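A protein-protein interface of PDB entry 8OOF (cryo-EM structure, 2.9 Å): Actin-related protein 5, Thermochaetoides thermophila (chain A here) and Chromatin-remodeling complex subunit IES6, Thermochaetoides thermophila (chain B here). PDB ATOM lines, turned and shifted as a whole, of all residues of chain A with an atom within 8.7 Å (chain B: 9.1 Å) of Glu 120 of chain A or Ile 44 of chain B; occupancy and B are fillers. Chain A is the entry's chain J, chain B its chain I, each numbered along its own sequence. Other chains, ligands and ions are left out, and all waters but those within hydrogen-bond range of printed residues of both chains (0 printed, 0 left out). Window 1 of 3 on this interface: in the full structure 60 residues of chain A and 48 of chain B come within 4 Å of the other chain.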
ATOM      1  N   SER A  65      19.183 -10.622 -13.871  1.00  0.00           N
ATOM      2  CA  SER A  65      19.320 -10.797 -12.429  1.00  0.00           C
ATOM      3  C   SER A  65      18.925  -9.550 -11.656  1.00  0.00           C
ATOM      4  O   SER A  65      18.535  -9.646 -10.488  1.00  0.00           O
ATOM      5  CB  SER A  65      20.756 -11.182 -12.083  1.00  0.00           C
ATOM      6  OG  SER A  65      21.197 -12.265 -12.877  1.00  0.00           O
ATOM      7  N   PRO A  84      13.626 -10.311  -9.977  1.00  0.00           N
ATOM      8  CA  PRO A  84      13.381 -11.762  -9.889  1.00  0.00           C
ATOM      9  C   PRO A  84      13.253 -12.273  -8.456  1.00  0.00           C
ATOM     10  O   PRO A  84      13.961 -13.187  -8.026  1.00  0.00           O
ATOM     11  CB  PRO A  84      14.606 -12.340 -10.608  1.00  0.00           C
ATOM     12  CG  PRO A  84      15.679 -11.378 -10.301  1.00  0.00           C
ATOM     13  CD  PRO A  84      15.020 -10.021 -10.341  1.00  0.00           C
ATOM     14  N   ASN A 117      15.275 -14.600  -3.780  1.00  0.00           N
ATOM     15  CA  ASN A 117      15.639 -14.226  -5.140  1.00  0.00           C
ATOM     16  C   ASN A 117      15.968 -15.473  -5.951  1.00  0.00           C
ATOM     17  O   ASN A 117      16.519 -16.446  -5.428  1.00  0.00           O
ATOM     18  CB  ASN A 117      16.832 -13.257  -5.134  1.00  0.00           C
ATOM     19  CG  ASN A 117      17.123 -12.669  -6.497  1.00  0.00           C
ATOM     20  OD1 ASN A 117      17.444 -13.384  -7.442  1.00  0.00           O
ATOM     21  ND2 ASN A 117      17.011 -11.352  -6.604  1.00  0.00           N
ATOM     22  N   ALA A 118      15.615 -15.433  -7.241  1.00  0.00           N
ATOM     23  CA  ALA A 118      15.825 -16.584  -8.114  1.00  0.00           C
ATOM     24  C   ALA A 118      17.299 -16.864  -8.376  1.00  0.00           C
ATOM     25  O   ALA A 118      17.684 -18.024  -8.556  1.00  0.00           O
ATOM     26  CB  ALA A 118      15.090 -16.373  -9.435  1.00  0.00           C
ATOM     27  N   PHE A 119      18.131 -15.833  -8.414  1.00  0.00           N
ATOM     28  CA  PHE A 119      19.529 -15.993  -8.780  1.00  0.00           C
ATOM     29  C   PHE A 119      20.404 -16.181  -7.550  1.00  0.00           C
ATOM     30  O   PHE A 119      20.120 -15.654  -6.472  1.00  0.00           O
ATOM     31  CB  PHE A 119      20.015 -14.790  -9.587  1.00  0.00           C
ATOM     32  CG  PHE A 119      19.329 -14.633 -10.908  1.00  0.00           C
ATOM     33  CD1 PHE A 119      18.109 -13.987 -10.999  1.00  0.00           C
ATOM     34  CD2 PHE A 119      19.906 -15.123 -12.062  1.00  0.00           C
ATOM     35  CE1 PHE A 119      17.480 -13.843 -12.214  1.00  0.00           C
ATOM     36  CE2 PHE A 119      19.282 -14.974 -13.278  1.00  0.00           C
ATOM     37  CZ  PHE A 119      18.068 -14.334 -13.353  1.00  0.00           C
ATOM     38  N   GLU A 120      21.481 -16.940  -7.722  1.00  0.00           N
ATOM     39  CA  GLU A 120      22.548 -16.958  -6.732  1.00  0.00           C
ATOM     40  C   GLU A 120      23.267 -15.616  -6.734  1.00  0.00           C
ATOM     41  O   GLU A 120      23.738 -15.159  -7.781  1.00  0.00           O
ATOM     42  CB  GLU A 120      23.525 -18.092  -7.018  1.00  0.00           C
ATOM     43  CG  GLU A 120      24.732 -18.086  -6.108  1.00  0.00           C
ATOM     44  CD  GLU A 120      25.467 -19.403  -6.119  1.00  0.00           C
ATOM     45  OE1 GLU A 120      24.816 -20.439  -6.361  1.00  0.00           O
ATOM     46  OE2 GLU A 120      26.692 -19.406  -5.879  1.00  0.00           O
ATOM     47  N   ALA A 121      23.338 -14.982  -5.566  1.00  0.00           N
ATOM     48  CA  ALA A 121      23.776 -13.596  -5.480  1.00  0.00           C
ATOM     49  C   ALA A 121      25.199 -13.434  -5.998  1.00  0.00           C
ATOM     50  O   ALA A 121      26.104 -14.179  -5.617  1.00  0.00           O
ATOM     51  CB  ALA A 121      23.683 -13.106  -4.036  1.00  0.00           C
ATOM     52  N   GLY A 122      25.387 -12.449  -6.873  1.00  0.00           N
ATOM     53  CA  GLY A 122      26.646 -12.265  -7.561  1.00  0.00           C
ATOM     54  C   GLY A 122      26.926 -13.230  -8.685  1.00  0.00           C
ATOM     55  O   GLY A 122      28.092 -13.420  -9.043  1.00  0.00           O
ATOM     56  N   THR A 123      25.898 -13.856  -9.250  1.00  0.00           N
ATOM     57  CA  THR A 123      26.049 -14.721 -10.410  1.00  0.00           C
ATOM     58  C   THR A 123      24.912 -14.442 -11.380  1.00  0.00           C
ATOM     59  O   THR A 123      23.902 -13.830 -11.028  1.00  0.00           O
ATOM     60  CB  THR A 123      26.068 -16.215 -10.038  1.00  0.00           C
ATOM     61  OG1 THR A 123      24.731 -16.670  -9.797  1.00  0.00           O
ATOM     62  CG2 THR A 123      26.930 -16.486  -8.814  1.00  0.00           C
ATOM     63  N   GLY A 124      25.102 -14.874 -12.620  1.00  0.00           N
ATOM     64  CA  GLY A 124      24.096 -14.755 -13.650  1.00  0.00           C
ATOM     65  C   GLY A 124      23.204 -15.964 -13.781  1.00  0.00           C
ATOM     66  O   GLY A 124      22.385 -16.023 -14.705  1.00  0.00           O
ATOM     67  N   ILE A 125      23.332 -16.927 -12.879  1.00  0.00           N
ATOM     68  CA  ILE A 125      22.719 -18.237 -13.021  1.00  0.00           C
ATOM     69  C   ILE A 125      21.515 -18.323 -12.095  1.00  0.00           C
ATOM     70  O   ILE A 125      21.607 -17.981 -10.909  1.00  0.00           O
ATOM     71  CB  ILE A 125      23.733 -19.351 -12.718  1.00  0.00           C
ATOM     72  CG1 ILE A 125      24.761 -19.430 -13.843  1.00  0.00           C
ATOM     73  CG2 ILE A 125      23.030 -20.676 -12.552  1.00  0.00           C
ATOM     74  CD1 ILE A 125      26.078 -20.019 -13.417  1.00  0.00           C
ATOM     75  N   VAL A 126      20.384 -18.768 -12.639  1.00  0.00           N
ATOM     76  CA  VAL A 126      19.214 -19.061 -11.824  1.00  0.00           C
ATOM     77  C   VAL A 126      19.482 -20.292 -10.971  1.00  0.00           C
ATOM     78  O   VAL A 126      20.038 -21.292 -11.442  1.00  0.00           O
ATOM     79  CB  VAL A 126      17.975 -19.259 -12.711  1.00  0.00           C
ATOM     80  CG1 VAL A 126      16.770 -19.600 -11.863  1.00  0.00           C
ATOM     81  CG2 VAL A 126      17.707 -18.020 -13.528  1.00  0.00           C
ATOM     82  N   SER A 127      19.095 -20.219  -9.702  1.00  0.00           N
ATOM     83  CA  SER A 127      19.396 -21.281  -8.748  1.00  0.00           C
ATOM     84  C   SER A 127      18.241 -21.628  -7.818  1.00  0.00           C
ATOM     85  O   SER A 127      18.178 -22.772  -7.359  1.00  0.00           O
ATOM     86  CB  SER A 127      20.622 -20.916  -7.905  1.00  0.00           C
ATOM     87  OG  SER A 127      20.820 -21.864  -6.873  1.00  0.00           O
ATOM     88  N   ASN A 128      17.337 -20.700  -7.512  1.00  0.00           N
ATOM     89  CA  ASN A 128      16.114 -20.999  -6.769  1.00  0.00           C
ATOM     90  C   ASN A 128      14.968 -21.103  -7.770  1.00  0.00           C
ATOM     91  O   ASN A 128      14.348 -20.111  -8.149  1.00  0.00           O
ATOM     92  CB  ASN A 128      15.852 -19.933  -5.712  1.00  0.00           C
ATOM     93  CG  ASN A 128      16.994 -19.800  -4.729  1.00  0.00           C
ATOM     94  OD1 ASN A 128      17.417 -20.780  -4.115  1.00  0.00           O
ATOM     95  ND2 ASN A 128      17.515 -18.587  -4.588  1.00  0.00           N
ATOM     96  N   TRP A 129      14.698 -22.338  -8.198  1.00  0.00           N
ATOM     97  CA  TRP A 129      13.753 -22.593  -9.280  1.00  0.00           C
ATOM     98  C   TRP A 129      12.303 -22.415  -8.849  1.00  0.00           C
ATOM     99  O   TRP A 129      11.458 -22.041  -9.667  1.00  0.00           O
ATOM    100  CB  TRP A 129      13.983 -23.992  -9.838  1.00  0.00           C
ATOM    101  CG  TRP A 129      15.274 -24.069 -10.558  1.00  0.00           C
ATOM    102  CD1 TRP A 129      16.410 -24.691 -10.141  1.00  0.00           C
ATOM    103  CD2 TRP A 129      15.593 -23.432 -11.796  1.00  0.00           C
ATOM    104  NE1 TRP A 129      17.410 -24.514 -11.065  1.00  0.00           N
ATOM    105  CE2 TRP A 129      16.933 -23.738 -12.089  1.00  0.00           C
ATOM    106  CE3 TRP A 129      14.869 -22.645 -12.696  1.00  0.00           C
ATOM    107  CZ2 TRP A 129      17.560 -23.290 -13.241  1.00  0.00           C
ATOM    108  CZ3 TRP A 129      15.493 -22.202 -13.834  1.00  0.00           C
ATOM    109  CH2 TRP A 129      16.825 -22.524 -14.099  1.00  0.00           C
ATOM    110  N   ASN A 164      26.063 -20.515 -19.727  1.00  0.00           N
ATOM    111  CA  ASN A 164      25.063 -20.950 -18.761  1.00  0.00           C
ATOM    112  C   ASN A 164      25.164 -22.448 -18.506  1.00  0.00           C
ATOM    113  O   ASN A 164      25.383 -23.237 -19.427  1.00  0.00           O
ATOM    114  CB  ASN A 164      23.663 -20.595 -19.256  1.00  0.00           C
ATOM    115  CG  ASN A 164      22.597 -20.876 -18.225  1.00  0.00           C
ATOM    116  OD1 ASN A 164      22.837 -20.763 -17.027  1.00  0.00           O
ATOM    117  ND2 ASN A 164      21.410 -21.238 -18.684  1.00  0.00           N
ATOM    118  N   LEU A 165      25.018 -22.831 -17.244  1.00  0.00           N
ATOM    119  CA  LEU A 165      25.282 -24.207 -16.853  1.00  0.00           C
ATOM    120  C   LEU A 165      24.226 -25.141 -17.442  1.00  0.00           C
ATOM    121  O   LEU A 165      23.046 -24.785 -17.500  1.00  0.00           O
ATOM    122  CB  LEU A 165      25.314 -24.341 -15.333  1.00  0.00           C
ATOM    123  CG  LEU A 165      26.366 -23.505 -14.607  1.00  0.00           C
ATOM    124  CD1 LEU A 165      26.227 -23.675 -13.107  1.00  0.00           C
ATOM    125  CD2 LEU A 165      27.760 -23.895 -15.060  1.00  0.00           C
ATOM    126  N   TYR A 167      22.789 -27.882 -16.270  1.00  0.00           N
ATOM    127  CA  TYR A 167      21.739 -28.158 -15.294  1.00  0.00           C
ATOM    128  C   TYR A 167      20.760 -26.999 -15.165  1.00  0.00           C
ATOM    129  O   TYR A 167      19.553 -27.213 -15.013  1.00  0.00           O
ATOM    130  CB  TYR A 167      22.359 -28.470 -13.936  1.00  0.00           C
ATOM    131  CG  TYR A 167      21.335 -28.705 -12.855  1.00  0.00           C
ATOM    132  CD1 TYR A 167      20.698 -29.929 -12.730  1.00  0.00           C
ATOM    133  CD2 TYR A 167      20.991 -27.694 -11.971  1.00  0.00           C
ATOM    134  CE1 TYR A 167      19.755 -30.139 -11.751  1.00  0.00           C
ATOM    135  CE2 TYR A 167      20.053 -27.896 -10.990  1.00  0.00           C
ATOM    136  CZ  TYR A 167      19.435 -29.120 -10.886  1.00  0.00           C
ATOM    137  OH  TYR A 167      18.501 -29.325  -9.902  1.00  0.00           O
ATOM    138  N   SER A 168      21.259 -25.766 -15.206  1.00  0.00           N
ATOM    139  CA  SER A 168      20.372 -24.611 -15.128  1.00  0.00           C
ATOM    140  C   SER A 168      19.483 -24.506 -16.361  1.00  0.00           C
ATOM    141  O   SER A 168      18.293 -24.199 -16.249  1.00  0.00           O
ATOM    142  CB  SER A 168      21.189 -23.338 -14.946  1.00  0.00           C
ATOM    143  OG  SER A 168      22.006 -23.435 -13.796  1.00  0.00           O
ATOM    144  N   TYR A 210      24.421  -6.646 -13.878  1.00  0.00           N
ATOM    145  CA  TYR A 210      24.352  -6.933 -12.450  1.00  0.00           C
ATOM    146  C   TYR A 210      25.309  -8.054 -12.066  1.00  0.00           C
ATOM    147  O   TYR A 210      26.045  -7.947 -11.080  1.00  0.00           O
ATOM    148  CB  TYR A 210      22.920  -7.313 -12.086  1.00  0.00           C
ATOM    149  CG  TYR A 210      22.481  -6.979 -10.685  1.00  0.00           C
ATOM    150  CD1 TYR A 210      22.475  -5.670 -10.232  1.00  0.00           C
ATOM    151  CD2 TYR A 210      22.039  -7.971  -9.825  1.00  0.00           C
ATOM    152  CE1 TYR A 210      22.076  -5.364  -8.956  1.00  0.00           C
ATOM    153  CE2 TYR A 210      21.624  -7.673  -8.551  1.00  0.00           C
ATOM    154  CZ  TYR A 210      21.647  -6.370  -8.118  1.00  0.00           C
ATOM    155  OH  TYR A 210      21.211  -6.072  -6.849  1.00  0.00           O
ATOM    156  N   SER A 211      25.306  -9.143 -12.832  1.00  0.00           N
ATOM    157  CA  SER A 211      25.987 -10.357 -12.396  1.00  0.00           C
ATOM    158  C   SER A 211      27.499 -10.292 -12.577  1.00  0.00           C
ATOM    159  O   SER A 211      28.247 -10.846 -11.766  1.00  0.00           O
ATOM    160  CB  SER A 211      25.431 -11.561 -13.151  1.00  0.00           C
ATOM    161  OG  SER A 211      25.533 -11.383 -14.555  1.00  0.00           O
ATOM    162  N   ARG A 230      35.086 -13.529 -18.579  1.00  0.00           N
ATOM    163  CA  ARG A 230      34.228 -12.956 -17.548  1.00  0.00           C
ATOM    164  C   ARG A 230      35.057 -12.384 -16.405  1.00  0.00           C
ATOM    165  O   ARG A 230      36.074 -12.963 -16.014  1.00  0.00           O
ATOM    166  CB  ARG A 230      33.270 -14.014 -16.995  1.00  0.00           C
ATOM    167  CG  ARG A 230      32.215 -13.476 -16.049  1.00  0.00           C
ATOM    168  CD  ARG A 230      31.279 -14.576 -15.612  1.00  0.00           C
ATOM    169  NE  ARG A 230      31.978 -15.578 -14.820  1.00  0.00           N
ATOM    170  CZ  ARG A 230      32.051 -16.862 -15.134  1.00  0.00           C
ATOM    171  NH1 ARG A 230      31.403 -17.358 -16.174  1.00  0.00           N
ATOM    172  NH2 ARG A 230      32.780 -17.674 -14.376  1.00  0.00           N
ATOM    173  N   TRP A 236      25.896  -5.545  -9.047  1.00  0.00           N
ATOM    174  CA  TRP A 236      25.620  -6.104  -7.730  1.00  0.00           C
ATOM    175  C   TRP A 236      26.819  -5.930  -6.808  1.00  0.00           C
ATOM    176  O   TRP A 236      26.689  -5.444  -5.680  1.00  0.00           O
ATOM    177  CB  TRP A 236      25.270  -7.585  -7.854  1.00  0.00           C
ATOM    178  CG  TRP A 236      24.929  -8.220  -6.548  1.00  0.00           C
ATOM    179  CD1 TRP A 236      23.742  -8.136  -5.892  1.00  0.00           C
ATOM    180  CD2 TRP A 236      25.796  -8.991  -5.712  1.00  0.00           C
ATOM    181  NE1 TRP A 236      23.800  -8.833  -4.715  1.00  0.00           N
ATOM    182  CE2 TRP A 236      25.055  -9.364  -4.578  1.00  0.00           C
ATOM    183  CE3 TRP A 236      27.124  -9.407  -5.814  1.00  0.00           C
ATOM    184  CZ2 TRP A 236      25.594 -10.134  -3.555  1.00  0.00           C
ATOM    185  CZ3 TRP A 236      27.656 -10.177  -4.801  1.00  0.00           C
ATOM    186  CH2 TRP A 236      26.892 -10.531  -3.686  1.00  0.00           C
ATOM    187  N   HIS A 237      27.992  -6.346  -7.283  1.00  0.00           N
ATOM    188  CA  HIS A 237      29.230  -6.242  -6.521  1.00  0.00           C
ATOM    189  C   HIS A 237      29.577  -4.799  -6.174  1.00  0.00           C
ATOM    190  O   HIS A 237      30.139  -4.532  -5.108  1.00  0.00           O
ATOM    191  CB  HIS A 237      30.363  -6.877  -7.315  1.00  0.00           C
ATOM    192  CG  HIS A 237      30.102  -8.294  -7.715  1.00  0.00           C
ATOM    193  ND1 HIS A 237      30.633  -9.368  -7.037  1.00  0.00           N
ATOM    194  CD2 HIS A 237      29.360  -8.814  -8.720  1.00  0.00           C
ATOM    195  CE1 HIS A 237      30.241 -10.488  -7.613  1.00  0.00           C
ATOM    196  NE2 HIS A 237      29.464 -10.180  -8.635  1.00  0.00           N
ATOM    197  N   ASN B  41      16.816 -27.312  -6.315  1.00  0.00           N
ATOM    198  CA  ASN B  41      17.587 -26.104  -6.020  1.00  0.00           C
ATOM    199  C   ASN B  41      19.001 -26.474  -5.581  1.00  0.00           C
ATOM    200  O   ASN B  41      19.206 -26.956  -4.464  1.00  0.00           O
ATOM    201  CB  ASN B  41      16.890 -25.280  -4.944  1.00  0.00           C
ATOM    202  CG  ASN B  41      15.655 -24.579  -5.457  1.00  0.00           C
ATOM    203  OD1 ASN B  41      15.200 -24.839  -6.566  1.00  0.00           O
ATOM    204  ND2 ASN B  41      15.112 -23.674  -4.655  1.00  0.00           N
ATOM    205  N   LYS B  42      19.979 -26.241  -6.454  1.00  0.00           N
ATOM    206  CA  LYS B  42      21.376 -26.548  -6.180  1.00  0.00           C
ATOM    207  C   LYS B  42      22.240 -25.329  -6.474  1.00  0.00           C
ATOM    208  O   LYS B  42      21.969 -24.575  -7.412  1.00  0.00           O
ATOM    209  CB  LYS B  42      21.863 -27.754  -6.987  1.00  0.00           C
ATOM    210  CG  LYS B  42      21.142 -29.040  -6.639  1.00  0.00           C
ATOM    211  CD  LYS B  42      21.826 -30.249  -7.240  1.00  0.00           C
ATOM    212  CE  LYS B  42      21.753 -30.239  -8.746  1.00  0.00           C
ATOM    213  NZ  LYS B  42      22.181 -31.540  -9.320  1.00  0.00           N
ATOM    214  N   THR B  43      23.273 -25.135  -5.655  1.00  0.00           N
ATOM    215  CA  THR B  43      24.210 -24.035  -5.821  1.00  0.00           C
ATOM    216  C   THR B  43      25.253 -24.352  -6.892  1.00  0.00           C
ATOM    217  O   THR B  43      25.469 -25.506  -7.268  1.00  0.00           O
ATOM    218  CB  THR B  43      24.904 -23.717  -4.496  1.00  0.00           C
ATOM    219  OG1 THR B  43      25.547 -24.894  -3.995  1.00  0.00           O
ATOM    220  CG2 THR B  43      23.892 -23.222  -3.476  1.00  0.00           C
ATOM    221  N   ILE B  44      25.904 -23.289  -7.376  1.00  0.00           N
ATOM    222  CA  ILE B  44      26.883 -23.400  -8.459  1.00  0.00           C
ATOM    223  C   ILE B  44      27.969 -24.410  -8.122  1.00  0.00           C
ATOM    224  O   ILE B  44      28.362 -25.226  -8.965  1.00  0.00           O
ATOM    225  CB  ILE B  44      27.492 -22.020  -8.771  1.00  0.00           C
ATOM    226  CG1 ILE B  44      26.404 -20.990  -9.081  1.00  0.00           C
ATOM    227  CG2 ILE B  44      28.475 -22.120  -9.919  1.00  0.00           C
ATOM    228  CD1 ILE B  44      25.295 -21.507  -9.951  1.00  0.00           C
ATOM    229  N   LYS B  45      28.479 -24.366  -6.891  1.00  0.00           N
ATOM    230  CA  LYS B  45      29.492 -25.330  -6.471  1.00  0.00           C
ATOM    231  C   LYS B  45      28.964 -26.756  -6.547  1.00  0.00           C
ATOM    232  O   LYS B  45      29.671 -27.665  -6.996  1.00  0.00           O
ATOM    233  CB  LYS B  45      29.969 -25.005  -5.058  1.00  0.00           C
ATOM    234  CG  LYS B  45      31.089 -25.904  -4.561  1.00  0.00           C
ATOM    235  CD  LYS B  45      31.523 -25.524  -3.158  1.00  0.00           C
ATOM    236  CE  LYS B  45      32.606 -26.457  -2.648  1.00  0.00           C
ATOM    237  NZ  LYS B  45      33.006 -26.134  -1.250  1.00  0.00           N
ATOM    238  N   ALA B  46      27.725 -26.970  -6.104  1.00  0.00           N
ATOM    239  CA  ALA B  46      27.112 -28.291  -6.199  1.00  0.00           C
ATOM    240  C   ALA B  46      26.921 -28.712  -7.653  1.00  0.00           C
ATOM    241  O   ALA B  46      27.224 -29.851  -8.024  1.00  0.00           O
ATOM    242  CB  ALA B  46      25.777 -28.300  -5.457  1.00  0.00           C
ATOM    243  N   ILE B  47      26.414 -27.804  -8.489  1.00  0.00           N
ATOM    244  CA  ILE B  47      26.223 -28.113  -9.904  1.00  0.00           C
ATOM    245  C   ILE B  47      27.552 -28.449 -10.569  1.00  0.00           C
ATOM    246  O   ILE B  47      27.681 -29.469 -11.255  1.00  0.00           O
ATOM    247  CB  ILE B  47      25.525 -26.943 -10.620  1.00  0.00           C
ATOM    248  CG1 ILE B  47      24.123 -26.728 -10.058  1.00  0.00           C
ATOM    249  CG2 ILE B  47      25.466 -27.202 -12.108  1.00  0.00           C
ATOM    250  CD1 ILE B  47      23.546 -25.379 -10.393  1.00  0.00           C
ATOM    251  N   LEU B  48      28.561 -27.599 -10.375  1.00  0.00           N
ATOM    252  CA  LEU B  48      29.871 -27.862 -10.962  1.00  0.00           C
ATOM    253  C   LEU B  48      30.488 -29.136 -10.399  1.00  0.00           C
ATOM    254  O   LEU B  48      31.064 -29.937 -11.143  1.00  0.00           O
ATOM    255  CB  LEU B  48      30.798 -26.671 -10.730  1.00  0.00           C
ATOM    256  CG  LEU B  48      30.441 -25.395 -11.490  1.00  0.00           C
ATOM    257  CD1 LEU B  48      31.361 -24.263 -11.084  1.00  0.00           C
ATOM    258  CD2 LEU B  48      30.521 -25.639 -12.982  1.00  0.00           C
ATOM    259  N   GLY B  49      30.388 -29.333  -9.086  1.00  0.00           N
ATOM    260  CA  GLY B  49      30.931 -30.539  -8.482  1.00  0.00           C
ATOM    261  C   GLY B  49      30.268 -31.808  -8.983  1.00  0.00           C
ATOM    262  O   GLY B  49      30.932 -32.826  -9.192  1.00  0.00           O
ATOM    263  N   GLU B  50      28.951 -31.765  -9.190  1.00  0.00           N
ATOM    264  CA  GLU B  50      28.242 -32.906  -9.757  1.00  0.00           C
ATOM    265  C   GLU B  50      28.458 -33.049 -11.258  1.00  0.00           C
ATOM    266  O   GLU B  50      28.394 -34.167 -11.780  1.00  0.00           O
ATOM    267  CB  GLU B  50      26.748 -32.791  -9.458  1.00  0.00           C
ATOM    268  CG  GLU B  50      26.395 -32.995  -7.996  1.00  0.00           C
ATOM    269  CD  GLU B  50      24.916 -32.803  -7.723  1.00  0.00           C
ATOM    270  OE1 GLU B  50      24.170 -32.512  -8.680  1.00  0.00           O
ATOM    271  OE2 GLU B  50      24.503 -32.943  -6.553  1.00  0.00           O
ATOM    272  N   SER B  51      28.720 -31.951 -11.967  1.00  0.00           N
ATOM    273  CA  SER B  51      29.033 -32.065 -13.387  1.00  0.00           C
ATOM    274  C   SER B  51      30.425 -32.636 -13.619  1.00  0.00           C
ATOM    275  O   SER B  51      30.657 -33.302 -14.633  1.00  0.00           O
ATOM    276  CB  SER B  51      28.903 -30.703 -14.068  1.00  0.00           C
ATOM    277  OG  SER B  51      27.598 -30.174 -13.914  1.00  0.00           O
ATOM    278  N   GLN B  52      31.359 -32.383 -12.707  1.00  0.00           N
ATOM    279  CA  GLN B  52      32.716 -32.902 -12.837  1.00  0.00           C
ATOM    280  C   GLN B  52      32.730 -34.426 -12.818  1.00  0.00           C
ATOM    281  O   GLN B  52      32.077 -35.050 -11.982  1.00  0.00           O
ATOM    282  CB  GLN B  52      33.607 -32.356 -11.722  1.00  0.00           C
ATOM    283  CG  GLN B  52      35.060 -32.787 -11.823  1.00  0.00           C
ATOM    284  CD  GLN B  52      35.934 -32.129 -10.774  1.00  0.00           C
ATOM    285  OE1 GLN B  52      35.443 -31.415  -9.900  1.00  0.00           O
ATOM    286  NE2 GLN B  52      37.238 -32.369 -10.855  1.00  0.00           N
ATOM    287  N   THR B 155      32.634 -21.796 -20.484  1.00  0.00           N
ATOM    288  CA  THR B 155      32.210 -23.038 -19.856  1.00  0.00           C
ATOM    289  C   THR B 155      32.370 -22.905 -18.344  1.00  0.00           C
ATOM    290  O   THR B 155      32.650 -23.879 -17.645  1.00  0.00           O
ATOM    291  CB  THR B 155      33.023 -24.232 -20.387  1.00  0.00           C
ATOM    292  OG1 THR B 155      33.191 -24.090 -21.802  1.00  0.00           O
ATOM    293  CG2 THR B 155      32.298 -25.544 -20.126  1.00  0.00           C
ATOM    294  N   ASN B 156      32.192 -21.678 -17.852  1.00  0.00           N
ATOM    295  CA  ASN B 156      32.697 -21.270 -16.539  1.00  0.00           C
ATOM    296  C   ASN B 156      34.197 -21.543 -16.423  1.00  0.00           C
ATOM    297  O   ASN B 156      34.707 -21.929 -15.370  1.00  0.00           O
ATOM    298  CB  ASN B 156      31.910 -21.938 -15.412  1.00  0.00           C
ATOM    299  CG  ASN B 156      30.577 -21.255 -15.154  1.00  0.00           C
ATOM    300  OD1 ASN B 156      29.888 -20.842 -16.085  1.00  0.00           O
ATOM    301  ND2 ASN B 156      30.218 -21.116 -13.884  1.00  0.00           N
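Of the 14 printed residues of chain B, 7 touch a printed residue of chain A.
Printed residues of chain B that touch a printed residue of chain A: Asn 41, Lys 42, Thr 43, Ile 44, Ile 47, Leu 48 and Asn 156.
Hydrophobic or aromatic side chains of chain B within 4 Å of the printed part of chain A: Ile 44, Ile 47 and Leu 48.
Among the printed residues, 14 pairs touch across the chains.
O of Lys 42 of chain B is in hydrogen-bond range of OG of Ser 127 of chain A, 3.0 Å away.
OE1 of Glu 120 of chain A sits close to N of Ile 44 of chain B (3.2 Å).
OD1 of Asn 41 of chain B is in hydrogen-bond range of N of Trp 129 of chain A, at 3.0 Å.
Thr 43 of chain B touches Glu 120 of chain A.
Ile 125 of chain A touches Ile 44 of chain B.
Ser 127 of chain A touches Asn 41 of chain B.
Asn 128 of chain A touches Asn 41 of chain B.
CG2 of Ile 47 of chain B touches CD1 of Leu 165 of chain A (3.7 Å).
Leu 48 of chain B touches Leu 165 of chain A (CD2 to CD2, 3.9 Å).
Asn 156 of chain B touches Leu 165 of chain A (OD1 to CD2, 3.9 Å).
Tyr 167 of chain A touches Lys 42 of chain B (CZ to CE, 3.3 Å).
CD2 of Tyr 167 of chain A touches CD1 of Ile 47 of chain B, at 3.8 Å.
NH1 of Arg 230 of chain A touches OD1 of Asn 156 of chain B, at 3.8 Å.
Of chain B, only Thr 43 and Ile 44 come within 4 Å of Glu 120 of chain A.
No residue of chain B comes within 4 Å of Gly 122 of chain A.
Of the printed residues of chain B, Ser 127 of chain A touches Asn 41 and Lys 42.
Of the printed residues of chain A, Lys 42 of chain B touches Ser 127 and Tyr 167.
Thr 43 of chain B touches just one residue of chain A: Glu 120.
Ile 44 of chain B touches three residues of chain A.
Of the printed residues of chain A, Leu 48 of chain B touches Leu 165 (3.9 Å).
Printed residues of chain A within 4 Å of Asn 156 of chain B: Leu 165 and Arg 230.
The nearest printed residue of chain B that does not touch Ser 127 of chain A is Thr 43 of chain B (4.2 Å).
The backbone carbonyl oxygen (O) of Asn 117 of chain A is in hydrogen-bond range of the side-chain amide nitrogen (ND2) of Asn 128 of chain A (2.5 Å).
The backbone carbonyl oxygen of Ile 47 of chain B lies within hydrogen-bond range of the side-chain hydroxyl of Ser 51 of chain B (2.8 Å).
The side-chain carboxylate (OE2) of Glu 50 of chain B is in salt-bridge range of the side-chain amino group (NZ) of Lys 42 of chain B (3.9 Å).
OG1 of Thr 123 of chain A sits close to N of Ile 125 of chain A.
The backbone carbonyl oxygen (O) of Ile 125 of chain A sits at hydrogen-bond distance from the backbone NH (N) of Glu 120 of chain A, at 3.4 Å.
O of Ala 118 of chain A is in hydrogen-bond range of N of Asn 128 of chain A, 2.9 Å away.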
